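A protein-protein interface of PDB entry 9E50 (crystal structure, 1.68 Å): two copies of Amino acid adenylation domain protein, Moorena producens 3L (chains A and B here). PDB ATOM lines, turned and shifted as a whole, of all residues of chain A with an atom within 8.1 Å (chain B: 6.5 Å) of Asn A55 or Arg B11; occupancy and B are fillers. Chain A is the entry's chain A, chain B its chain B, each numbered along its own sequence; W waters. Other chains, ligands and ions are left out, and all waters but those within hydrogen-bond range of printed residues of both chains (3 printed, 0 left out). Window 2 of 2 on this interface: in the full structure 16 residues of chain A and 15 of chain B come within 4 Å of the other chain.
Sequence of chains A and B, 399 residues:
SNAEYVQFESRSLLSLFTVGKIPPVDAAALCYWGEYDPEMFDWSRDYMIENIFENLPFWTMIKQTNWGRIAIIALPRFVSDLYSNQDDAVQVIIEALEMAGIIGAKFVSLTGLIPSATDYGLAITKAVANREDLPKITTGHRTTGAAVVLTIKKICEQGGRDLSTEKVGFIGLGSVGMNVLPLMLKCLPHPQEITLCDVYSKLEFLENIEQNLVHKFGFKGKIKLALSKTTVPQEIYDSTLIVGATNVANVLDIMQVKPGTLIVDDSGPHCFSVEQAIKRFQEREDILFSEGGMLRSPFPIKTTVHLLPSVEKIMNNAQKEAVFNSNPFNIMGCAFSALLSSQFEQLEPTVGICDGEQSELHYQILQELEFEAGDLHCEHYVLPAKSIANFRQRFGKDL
Asn A55 touches just these residues of chain B: Arg B11 and Lys B21.
Arg B11 touches just these residues of chain A: Glu A54 (3.0 Å), Asn A55 (3.8 Å) and Leu A56 (3.96 Å).
No residue of chain A comes within 4 Å of Ser B10.
Of the printed residues of chain B, Glu A95 touches Val B19 and Lys B21.
Of the printed residues of chain A, Leu B16 touches Leu A56 (3.99 Å).
Of the printed residues of chain B, Glu A54 touches Arg B11 (3.0 Å).
Of the printed residues of chain A, Ser B15 touches Leu A56 (3.9 Å).
Of the printed residues of chain B, Leu A56 touches Arg B11, Ser B15, Leu B16 and Val B19.
Ile A52 touches none of the printed residues of chain B.
The nearest printed residue of chain B that does not touch Glu A54 is Ser B12 (5.2 Å).
Water W3 lies within hydrogen-bond range of OE1 of Glu A54 (2.4 Å) and N of Ser B12 (2.9 Å).
Water W2 lies within hydrogen-bond range of O of Pro A57 and OG of Ser B15.
Water W1 lies within hydrogen-bond range of the side-chain carboxylate (OE1) of Glu A95 (2.7 Å), the side-chain amino group (NZ) of Lys B21 (2.8 Å) and the side-chain amide oxygen (OD1) of Asn A55 (3.0 Å).
Printed residues of chain A that touch a printed residue of chain B: Glu A54, Asn A55, Leu A56, Pro A57 and Glu A95.
Hydrophobic or aromatic side chains of chain A within 4 Å of the printed part of chain B: Leu A56 and Pro A57.
Of the 11 printed residues of chain B, 5 touch a printed residue of chain A.
Hydrophobic or aromatic side chains of chain B that line the printed part of chain A: Leu B16 and Val B19.
Among the printed residues, Asp or Glu carboxylates within 4 Å of a Lys or Arg side-chain nitrogen of the other chain: Glu A95 with Lys B21 (3.7 Å).
N of Glu A54 lies within hydrogen-bond range of O of Ile A49 (3.2 Å).
O of Ile A49 is in hydrogen-bond range of N of Asn A55, at 2.8 Å.
The guanidinium group (NH1) of Arg A77 lies within hydrogen-bond range of the side-chain amide oxygen (OD1) of Asn A55 (2.8 Å).
The backbone carbonyl oxygen (O) of Arg B11 lies within hydrogen-bond range of a ring nitrogen (ND1) of His B306 (3.3 Å).
N of Ser B15 sits at hydrogen-bond distance from OG of Ser B12.
N of Lys B21 sits at hydrogen-bond distance from O of Leu B16, 2.9 Å away.
The guanidinium group of Arg B11 is in hydrogen-bond range of the backbone carbonyl oxygen of Glu A54, at 3.0 Å.
The side-chain amino group of Lys B21 sits at hydrogen-bond distance from the backbone carbonyl oxygen of Asn A55 (3.0 Å).
NZ of Lys B21 is in salt-bridge range of OE1 of Glu A95.
No position is printed for both chains.
Of the 10 pairs that touch across the chains among the printed residues, none has its exchanged pair printed and touching as well.
Arg B11 touches Asn A55.
Leu A56 touches Arg B11.
Ser B15 touches Leu A56.
CD2 of Leu A56 touches CD2 of Leu B16, 3.99 Å away.
Val B19 touches Leu A56.
Val B19 touches Pro A57.
O of Glu A95 touches CG1 of Val B19 (3.6 Å).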
ATOM      1  N   ASP A  46       6.900 -14.356   2.928  1.00  0.00           N
ATOM      2  CA  ASP A  46       7.117 -13.570   4.139  1.00  0.00           C
ATOM      3  C   ASP A  46       8.176 -12.495   3.923  1.00  0.00           C
ATOM      4  O   ASP A  46       8.028 -11.364   4.405  1.00  0.00           O
ATOM      5  CB  ASP A  46       7.513 -14.481   5.299  1.00  0.00           C
ATOM      6  CG  ASP A  46       7.799 -13.707   6.577  1.00  0.00           C
ATOM      7  OD1 ASP A  46       6.869 -13.045   7.091  1.00  0.00           O
ATOM      8  OD2 ASP A  46       8.950 -13.759   7.068  1.00  0.00           O
ATOM      9  N   TYR A  47       9.253 -12.828   3.205  1.00  0.00           N
ATOM     10  CA  TYR A  47      10.296 -11.844   2.927  1.00  0.00           C
ATOM     11  C   TYR A  47       9.740 -10.662   2.142  1.00  0.00           C
ATOM     12  O   TYR A  47      10.063  -9.503   2.432  1.00  0.00           O
ATOM     13  CB  TYR A  47      11.447 -12.504   2.163  1.00  0.00           C
ATOM     14  CG  TYR A  47      12.619 -11.582   1.862  1.00  0.00           C
ATOM     15  CD1 TYR A  47      12.556 -10.652   0.826  1.00  0.00           C
ATOM     16  CD2 TYR A  47      13.797 -11.659   2.599  1.00  0.00           C
ATOM     17  CE1 TYR A  47      13.622  -9.814   0.545  1.00  0.00           C
ATOM     18  CE2 TYR A  47      14.873 -10.825   2.322  1.00  0.00           C
ATOM     19  CZ  TYR A  47      14.778  -9.906   1.293  1.00  0.00           C
ATOM     20  OH  TYR A  47      15.836  -9.071   1.007  1.00  0.00           O
ATOM     21  N   MET A  48       8.917 -10.934   1.132  1.00  0.00           N
ATOM     22  CA  MET A  48       8.400  -9.849   0.309  1.00  0.00           C
ATOM     23  C   MET A  48       7.460  -8.955   1.103  1.00  0.00           C
ATOM     24  O   MET A  48       7.507  -7.726   0.971  1.00  0.00           O
ATOM     25  CB  MET A  48       7.705 -10.418  -0.922  1.00  0.00           C
ATOM     26  CG  MET A  48       8.640 -11.273  -1.744  1.00  0.00           C
ATOM     27  SD  MET A  48       7.956 -11.716  -3.337  1.00  0.00           S
ATOM     28  CE  MET A  48       7.885 -10.112  -4.143  1.00  0.00           C
ATOM     29  N   ILE A  49       6.625  -9.549   1.957  1.00  0.00           N
ATOM     30  CA  ILE A  49       5.713  -8.753   2.773  1.00  0.00           C
ATOM     31  C   ILE A  49       6.496  -7.860   3.730  1.00  0.00           C
ATOM     32  O   ILE A  49       6.190  -6.670   3.885  1.00  0.00           O
ATOM     33  CB  ILE A  49       4.732  -9.671   3.527  1.00  0.00           C
ATOM     34  CG1 ILE A  49       3.737 -10.319   2.556  1.00  0.00           C
ATOM     35  CG2 ILE A  49       4.006  -8.900   4.617  1.00  0.00           C
ATOM     36  CD1 ILE A  49       2.789 -11.298   3.226  1.00  0.00           C
ATOM     37  N   GLU A  50       7.534  -8.408   4.367  1.00  0.00           N
ATOM     38  CA  GLU A  50       8.219  -7.683   5.434  1.00  0.00           C
ATOM     39  C   GLU A  50       9.276  -6.720   4.902  1.00  0.00           C
ATOM     40  O   GLU A  50       9.454  -5.631   5.460  1.00  0.00           O
ATOM     41  CB  GLU A  50       8.856  -8.673   6.414  1.00  0.00           C
ATOM     42  CG  GLU A  50       7.850  -9.492   7.206  1.00  0.00           C
ATOM     43  CD  GLU A  50       6.957  -8.635   8.082  1.00  0.00           C
ATOM     44  OE1 GLU A  50       7.444  -7.617   8.623  1.00  0.00           O
ATOM     45  OE2 GLU A  50       5.763  -8.976   8.225  1.00  0.00           O
ATOM     46  N   ASN A  51       9.994  -7.096   3.841  1.00  0.00           N
ATOM     47  CA  ASN A  51      11.134  -6.313   3.390  1.00  0.00           C
ATOM     48  C   ASN A  51      10.904  -5.554   2.092  1.00  0.00           C
ATOM     49  O   ASN A  51      11.602  -4.566   1.849  1.00  0.00           O
ATOM     50  CB  ASN A  51      12.370  -7.213   3.229  1.00  0.00           C
ATOM     51  CG  ASN A  51      12.868  -7.758   4.556  1.00  0.00           C
ATOM     52  OD1 ASN A  51      12.627  -7.170   5.611  1.00  0.00           O
ATOM     53  ND2 ASN A  51      13.565  -8.886   4.508  1.00  0.00           N
ATOM     54  N   ILE A  52       9.961  -5.973   1.255  1.00  0.00           N
ATOM     55  CA  ILE A  52       9.649  -5.248   0.029  1.00  0.00           C
ATOM     56  C   ILE A  52       8.427  -4.358   0.205  1.00  0.00           C
ATOM     57  O   ILE A  52       8.468  -3.171  -0.114  1.00  0.00           O
ATOM     58  CB  ILE A  52       9.470  -6.227  -1.152  1.00  0.00           C
ATOM     59  CG1 ILE A  52      10.728  -7.081  -1.320  1.00  0.00           C
ATOM     60  CG2 ILE A  52       9.166  -5.458  -2.435  1.00  0.00           C
ATOM     61  CD1 ILE A  52      10.692  -7.981  -2.525  1.00  0.00           C
ATOM     62  N   PHE A  53       7.332  -4.914   0.724  1.00  0.00           N
ATOM     63  CA  PHE A  53       6.148  -4.116   1.024  1.00  0.00           C
ATOM     64  C   PHE A  53       6.236  -3.417   2.375  1.00  0.00           C
ATOM     65  O   PHE A  53       5.381  -2.573   2.671  1.00  0.00           O
ATOM     66  CB  PHE A  53       4.884  -4.986   1.001  1.00  0.00           C
ATOM     67  CG  PHE A  53       4.719  -5.806  -0.250  1.00  0.00           C
ATOM     68  CD1 PHE A  53       5.206  -5.353  -1.470  1.00  0.00           C
ATOM     69  CD2 PHE A  53       4.072  -7.034  -0.204  1.00  0.00           C
ATOM     70  CE1 PHE A  53       5.058  -6.109  -2.613  1.00  0.00           C
ATOM     71  CE2 PHE A  53       3.915  -7.797  -1.351  1.00  0.00           C
ATOM     72  CZ  PHE A  53       4.412  -7.330  -2.558  1.00  0.00           C
ATOM     73  N   GLU A  54       7.229  -3.764   3.198  1.00  0.00           N
ATOM     74  CA  GLU A  54       7.453  -3.179   4.522  1.00  0.00           C
ATOM     75  C   GLU A  54       6.256  -3.346   5.458  1.00  0.00           C
ATOM     76  O   GLU A  54       6.159  -2.645   6.474  1.00  0.00           O
ATOM     77  CB  GLU A  54       7.841  -1.699   4.409  1.00  0.00           C
ATOM     78  CG  GLU A  54       9.085  -1.469   3.554  1.00  0.00           C
ATOM     79  CD  GLU A  54       9.334  -0.001   3.231  1.00  0.00           C
ATOM     80  OE1 GLU A  54       8.487   0.850   3.579  1.00  0.00           O
ATOM     81  OE2 GLU A  54      10.383   0.299   2.621  1.00  0.00           O
ATOM     82  N   ASN A  55       5.346  -4.273   5.148  1.00  0.00           N
ATOM     83  CA  ASN A  55       4.141  -4.498   5.948  1.00  0.00           C
ATOM     84  C   ASN A  55       3.332  -3.213   6.108  1.00  0.00           C
ATOM     85  O   ASN A  55       2.658  -3.011   7.119  1.00  0.00           O
ATOM     86  CB  ASN A  55       4.487  -5.091   7.320  1.00  0.00           C
ATOM     87  CG  ASN A  55       3.311  -5.803   7.967  1.00  0.00           C
ATOM     88  OD1 ASN A  55       2.353  -6.180   7.294  1.00  0.00           O
ATOM     89  ND2 ASN A  55       3.384  -5.998   9.280  1.00  0.00           N
ATOM     90  N   LEU A  56       3.397  -2.334   5.108  1.00  0.00           N
ATOM     91  CA  LEU A  56       2.721  -1.048   5.157  1.00  0.00           C
ATOM     92  C   LEU A  56       1.914  -0.823   3.887  1.00  0.00           C
ATOM     93  O   LEU A  56       2.364  -1.183   2.792  1.00  0.00           O
ATOM     94  CB  LEU A  56       3.734   0.097   5.314  1.00  0.00           C
ATOM     95  CG  LEU A  56       4.379   0.271   6.687  1.00  0.00           C
ATOM     96  CD1 LEU A  56       5.599   1.170   6.573  1.00  0.00           C
ATOM     97  CD2 LEU A  56       3.374   0.863   7.653  1.00  0.00           C
ATOM     98  N   PRO A  57       0.733  -0.220   3.993  1.00  0.00           N
ATOM     99  CA  PRO A  57       0.041   0.230   2.784  1.00  0.00           C
ATOM    100  C   PRO A  57       0.878   1.277   2.074  1.00  0.00           C
ATOM    101  O   PRO A  57       1.630   2.029   2.701  1.00  0.00           O
ATOM    102  CB  PRO A  57      -1.264   0.823   3.317  1.00  0.00           C
ATOM    103  CG  PRO A  57      -0.926   1.268   4.671  1.00  0.00           C
ATOM    104  CD  PRO A  57       0.053   0.247   5.212  1.00  0.00           C
ATOM    105  N   PHE A  58       0.745   1.321   0.752  1.00  0.00           N
ATOM    106  CA  PHE A  58       1.574   2.187  -0.074  1.00  0.00           C
ATOM    107  C   PHE A  58       0.690   3.031  -0.978  1.00  0.00           C
ATOM    108  O   PHE A  58      -0.025   2.493  -1.829  1.00  0.00           O
ATOM    109  CB  PHE A  58       2.560   1.367  -0.900  1.00  0.00           C
ATOM    110  CG  PHE A  58       3.385   2.192  -1.831  1.00  0.00           C
ATOM    111  CD1 PHE A  58       4.251   3.152  -1.336  1.00  0.00           C
ATOM    112  CD2 PHE A  58       3.300   2.009  -3.201  1.00  0.00           C
ATOM    113  CE1 PHE A  58       5.015   3.922  -2.192  1.00  0.00           C
ATOM    114  CE2 PHE A  58       4.065   2.774  -4.066  1.00  0.00           C
ATOM    115  CZ  PHE A  58       4.925   3.731  -3.557  1.00  0.00           C
ATOM    116  N   ALA A  74      -2.053   0.531  -2.166  1.00  0.00           N
ATOM    117  CA  ALA A  74      -1.812  -0.907  -2.240  1.00  0.00           C
ATOM    118  C   ALA A  74      -1.615  -1.490  -0.846  1.00  0.00           C
ATOM    119  O   ALA A  74      -0.759  -1.025  -0.082  1.00  0.00           O
ATOM    120  CB  ALA A  74      -0.586  -1.202  -3.105  1.00  0.00           C
ATOM    121  N   LEU A  75      -2.402  -2.513  -0.521  1.00  0.00           N
ATOM    122  CA  LEU A  75      -2.163  -3.269   0.695  1.00  0.00           C
ATOM    123  C   LEU A  75      -0.873  -4.075   0.566  1.00  0.00           C
ATOM    124  O   LEU A  75      -0.547  -4.567  -0.516  1.00  0.00           O
ATOM    125  CB  LEU A  75      -3.321  -4.223   0.964  1.00  0.00           C
ATOM    126  CG  LEU A  75      -4.705  -3.578   0.992  1.00  0.00           C
ATOM    127  CD1 LEU A  75      -5.775  -4.648   1.143  1.00  0.00           C
ATOM    128  CD2 LEU A  75      -4.790  -2.567   2.121  1.00  0.00           C
ATOM    129  N   PRO A  76      -0.133  -4.245   1.668  1.00  0.00           N
ATOM    130  CA  PRO A  76       1.111  -5.027   1.664  1.00  0.00           C
ATOM    131  C   PRO A  76       0.875  -6.537   1.694  1.00  0.00           C
ATOM    132  O   PRO A  76       1.464  -7.261   2.500  1.00  0.00           O
ATOM    133  CB  PRO A  76       1.810  -4.548   2.940  1.00  0.00           C
ATOM    134  CG  PRO A  76       0.668  -4.239   3.867  1.00  0.00           C
ATOM    135  CD  PRO A  76      -0.404  -3.640   2.985  1.00  0.00           C
ATOM    136  N   ARG A  77       0.012  -7.016   0.801  1.00  0.00           N
ATOM    137  CA  ARG A  77      -0.394  -8.414   0.796  1.00  0.00           C
ATOM    138  C   ARG A  77      -0.592  -8.894  -0.635  1.00  0.00           C
ATOM    139  O   ARG A  77      -0.810  -8.103  -1.555  1.00  0.00           O
ATOM    140  CB  ARG A  77      -1.698  -8.634   1.588  1.00  0.00           C
ATOM    141  CG  ARG A  77      -1.602  -8.385   3.098  1.00  0.00           C
ATOM    142  CD  ARG A  77      -0.696  -9.397   3.795  1.00  0.00           C
ATOM    143  NE  ARG A  77      -0.725  -9.238   5.247  1.00  0.00           N
ATOM    144  CZ  ARG A  77       0.062  -8.416   5.928  1.00  0.00           C
ATOM    145  NH1 ARG A  77       0.959  -7.657   5.322  1.00  0.00           N
ATOM    146  NH2 ARG A  77      -0.051  -8.357   7.252  1.00  0.00           N
ATOM    147  N   ASP A  88      -6.317 -11.073   9.583  1.00  0.00           N
ATOM    148  CA  ASP A  88      -5.164 -10.294   9.146  1.00  0.00           C
ATOM    149  C   ASP A  88      -5.533  -9.360   8.001  1.00  0.00           C
ATOM    150  O   ASP A  88      -5.092  -8.202   7.966  1.00  0.00           O
ATOM    151  CB  ASP A  88      -4.039 -11.239   8.725  1.00  0.00           C
ATOM    152  CG  ASP A  88      -2.880 -10.515   8.070  1.00  0.00           C
ATOM    153  OD1 ASP A  88      -2.172  -9.764   8.769  1.00  0.00           O
ATOM    154  OD2 ASP A  88      -2.673 -10.700   6.850  1.00  0.00           O
ATOM    155  N   VAL A  92      -5.037  -5.226   8.156  1.00  0.00           N
ATOM    156  CA  VAL A  92      -4.253  -4.413   7.232  1.00  0.00           C
ATOM    157  C   VAL A  92      -5.148  -3.429   6.495  1.00  0.00           C
ATOM    158  O   VAL A  92      -4.710  -2.324   6.160  1.00  0.00           O
ATOM    159  CB  VAL A  92      -3.446  -5.285   6.247  1.00  0.00           C
ATOM    160  CG1 VAL A  92      -2.443  -6.149   6.998  1.00  0.00           C
ATOM    161  CG2 VAL A  92      -4.352  -6.147   5.400  1.00  0.00           C
ATOM    162  N   GLU A  95      -5.655  -0.491   8.810  1.00  0.00           N
ATOM    163  CA  GLU A  95      -4.469   0.355   8.744  1.00  0.00           C
ATOM    164  C   GLU A  95      -4.493   1.255   7.509  1.00  0.00           C
ATOM    165  O   GLU A  95      -4.212   2.457   7.601  1.00  0.00           O
ATOM    166  CB  GLU A  95      -3.213  -0.520   8.772  1.00  0.00           C
ATOM    167  CG  GLU A  95      -3.006  -1.188  10.133  1.00  0.00           C
ATOM    168  CD  GLU A  95      -1.998  -2.320  10.111  1.00  0.00           C
ATOM    169  OE1 GLU A  95      -1.258  -2.439   9.113  1.00  0.00           O
ATOM    170  OE2 GLU A  95      -1.951  -3.095  11.095  1.00  0.00           O
ATOM    171  N   GLU B   9      14.638   1.931  13.540  1.00  0.00           N
ATOM    172  CA  GLU B   9      13.468   1.564  12.755  1.00  0.00           C
ATOM    173  C   GLU B   9      13.805   1.718  11.277  1.00  0.00           C
ATOM    174  O   GLU B   9      14.151   2.816  10.827  1.00  0.00           O
ATOM    175  CB  GLU B   9      12.267   2.430  13.136  1.00  0.00           C
ATOM    176  CG  GLU B   9      11.030   2.153  12.311  1.00  0.00           C
ATOM    177  CD  GLU B   9      10.568   0.714  12.426  1.00  0.00           C
ATOM    178  OE1 GLU B   9      10.273   0.276  13.559  1.00  0.00           O
ATOM    179  OE2 GLU B   9      10.514   0.022  11.386  1.00  0.00           O
ATOM    180  N   SER B  10      13.700   0.618  10.527  1.00  0.00           N
ATOM    181  CA  SER B  10      14.013   0.640   9.102  1.00  0.00           C
ATOM    182  C   SER B  10      12.937   1.326   8.270  1.00  0.00           C
ATOM    183  O   SER B  10      13.228   1.775   7.156  1.00  0.00           O
ATOM    184  CB  SER B  10      14.223  -0.786   8.594  1.00  0.00           C
ATOM    185  OG  SER B  10      13.194  -1.646   9.049  1.00  0.00           O
ATOM    186  N   ARG B  11      11.717   1.430   8.778  1.00  0.00           N
ATOM    187  CA  ARG B  11      10.599   1.968   8.019  1.00  0.00           C
ATOM    188  C   ARG B  11      10.302   3.413   8.410  1.00  0.00           C
ATOM    189  O   ARG B  11      10.617   3.860   9.515  1.00  0.00           O
ATOM    190  CB  ARG B  11       9.356   1.100   8.224  1.00  0.00           C
ATOM    191  CG  ARG B  11       9.563  -0.354   7.814  1.00  0.00           C
ATOM    192  CD  ARG B  11       8.354  -1.195   8.156  1.00  0.00           C
ATOM    193  NE  ARG B  11       8.152  -1.298   9.595  1.00  0.00           N
ATOM    194  CZ  ARG B  11       7.092  -1.854  10.166  1.00  0.00           C
ATOM    195  NH1 ARG B  11       6.108  -2.369   9.444  1.00  0.00           N
ATOM    196  NH2 ARG B  11       7.009  -1.883  11.494  1.00  0.00           N
ATOM    197  N   SER B  12       9.674   4.132   7.477  1.00  0.00           N
ATOM    198  CA  SER B  12       9.325   5.537   7.675  1.00  0.00           C
ATOM    199  C   SER B  12       8.476   5.728   8.926  1.00  0.00           C
ATOM    200  O   SER B  12       7.439   5.078   9.093  1.00  0.00           O
ATOM    201  CB  SER B  12       8.571   6.057   6.446  1.00  0.00           C
ATOM    202  OG  SER B  12       7.855   7.252   6.723  1.00  0.00           O
ATOM    203  N   LEU B  13       8.915   6.635   9.806  1.00  0.00           N
ATOM    204  CA  LEU B  13       8.116   6.953  10.985  1.00  0.00           C
ATOM    205  C   LEU B  13       6.796   7.598  10.585  1.00  0.00           C
ATOM    206  O   LEU B  13       5.753   7.341  11.199  1.00  0.00           O
ATOM    207  CB  LEU B  13       8.902   7.867  11.932  1.00  0.00           C
ATOM    208  CG  LEU B  13      10.254   7.356  12.447  1.00  0.00           C
ATOM    209  CD1 LEU B  13      10.865   8.310  13.478  1.00  0.00           C
ATOM    210  CD2 LEU B  13      10.121   5.953  13.034  1.00  0.00           C
ATOM    211  N   LEU B  14       6.823   8.432   9.541  1.00  0.00           N
ATOM    212  CA  LEU B  14       5.597   9.037   9.028  1.00  0.00           C
ATOM    213  C   LEU B  14       4.602   7.971   8.579  1.00  0.00           C
ATOM    214  O   LEU B  14       3.408   8.050   8.891  1.00  0.00           O
ATOM    215  CB  LEU B  14       5.935   9.984   7.876  1.00  0.00           C
ATOM    216  CG  LEU B  14       4.781  10.816   7.315  1.00  0.00           C
ATOM    217  CD1 LEU B  14       4.267  11.791   8.364  1.00  0.00           C
ATOM    218  CD2 LEU B  14       5.212  11.553   6.055  1.00  0.00           C
ATOM    219  N   SER B  15       5.075   6.964   7.837  1.00  0.00           N
ATOM    220  CA  SER B  15       4.172   5.908   7.389  1.00  0.00           C
ATOM    221  C   SER B  15       3.630   5.115   8.568  1.00  0.00           C
ATOM    222  O   SER B  15       2.428   4.827   8.629  1.00  0.00           O
ATOM    223  CB  SER B  15       4.882   4.983   6.404  1.00  0.00           C
ATOM    224  OG  SER B  15       5.063   5.624   5.151  1.00  0.00           O
ATOM    225  N   LEU B  16       4.498   4.762   9.519  1.00  0.00           N
ATOM    226  CA  LEU B  16       4.047   4.023  10.695  1.00  0.00           C
ATOM    227  C   LEU B  16       3.001   4.810  11.472  1.00  0.00           C
ATOM    228  O   LEU B  16       2.036   4.235  11.990  1.00  0.00           O
ATOM    229  CB  LEU B  16       5.238   3.686  11.590  1.00  0.00           C
ATOM    230  CG  LEU B  16       6.216   2.635  11.068  1.00  0.00           C
ATOM    231  CD1 LEU B  16       7.432   2.569  11.972  1.00  0.00           C
ATOM    232  CD2 LEU B  16       5.530   1.280  10.985  1.00  0.00           C
ATOM    233  N   VAL B  19      -0.690   4.811   9.847  1.00  0.00           N
ATOM    234  CA  VAL B  19      -1.465   3.579   9.959  1.00  0.00           C
ATOM    235  C   VAL B  19      -1.759   3.220  11.411  1.00  0.00           C
ATOM    236  O   VAL B  19      -2.294   2.140  11.681  1.00  0.00           O
ATOM    237  CB  VAL B  19      -0.776   2.411   9.233  1.00  0.00           C
ATOM    238  CG1 VAL B  19      -0.658   2.723   7.759  1.00  0.00           C
ATOM    239  CG2 VAL B  19       0.599   2.116   9.833  1.00  0.00           C
ATOM    240  N   LYS B  21       0.407   2.621  13.843  1.00  0.00           N
ATOM    241  CA  LYS B  21       1.350   1.711  14.478  1.00  0.00           C
ATOM    242  C   LYS B  21       2.237   2.395  15.512  1.00  0.00           C
ATOM    243  O   LYS B  21       2.764   1.712  16.394  1.00  0.00           O
ATOM    244  CB  LYS B  21       2.203   1.008  13.419  1.00  0.00           C
ATOM    245  CG  LYS B  21       1.403  -0.014  12.622  1.00  0.00           C
ATOM    246  CD  LYS B  21       2.254  -0.780  11.628  1.00  0.00           C
ATOM    247  CE  LYS B  21       1.451  -1.903  10.990  1.00  0.00           C
ATOM    248  NZ  LYS B  21       2.283  -2.764  10.105  1.00  0.00           N
ATOM    249  N   HIS B 306      15.149   6.593  12.969  1.00  0.00           N
ATOM    250  CA  HIS B 306      14.987   6.211  11.572  1.00  0.00           C
ATOM    251  C   HIS B 306      15.993   7.015  10.761  1.00  0.00           C
ATOM    252  O   HIS B 306      15.804   8.217  10.545  1.00  0.00           O
ATOM    253  CB  HIS B 306      13.562   6.463  11.088  1.00  0.00           C
ATOM    254  CG  HIS B 306      13.361   6.176   9.633  1.00  0.00           C
ATOM    255  ND1 HIS B 306      13.677   4.963   9.064  1.00  0.00           N
ATOM    256  CD2 HIS B 306      12.879   6.948   8.631  1.00  0.00           C
ATOM    257  CE1 HIS B 306      13.401   4.999   7.773  1.00  0.00           C
ATOM    258  NE2 HIS B 306      12.917   6.193   7.484  1.00  0.00           N
HETATM  259  O   HOH W   1       0.478  -4.554   9.023  1.00  0.00           O
HETATM  260  O   HOH W   2       3.477   3.884   3.363  1.00  0.00           O
HETATM  261  O   HOH W   3       8.871   2.754   5.009  1.00  0.00           O
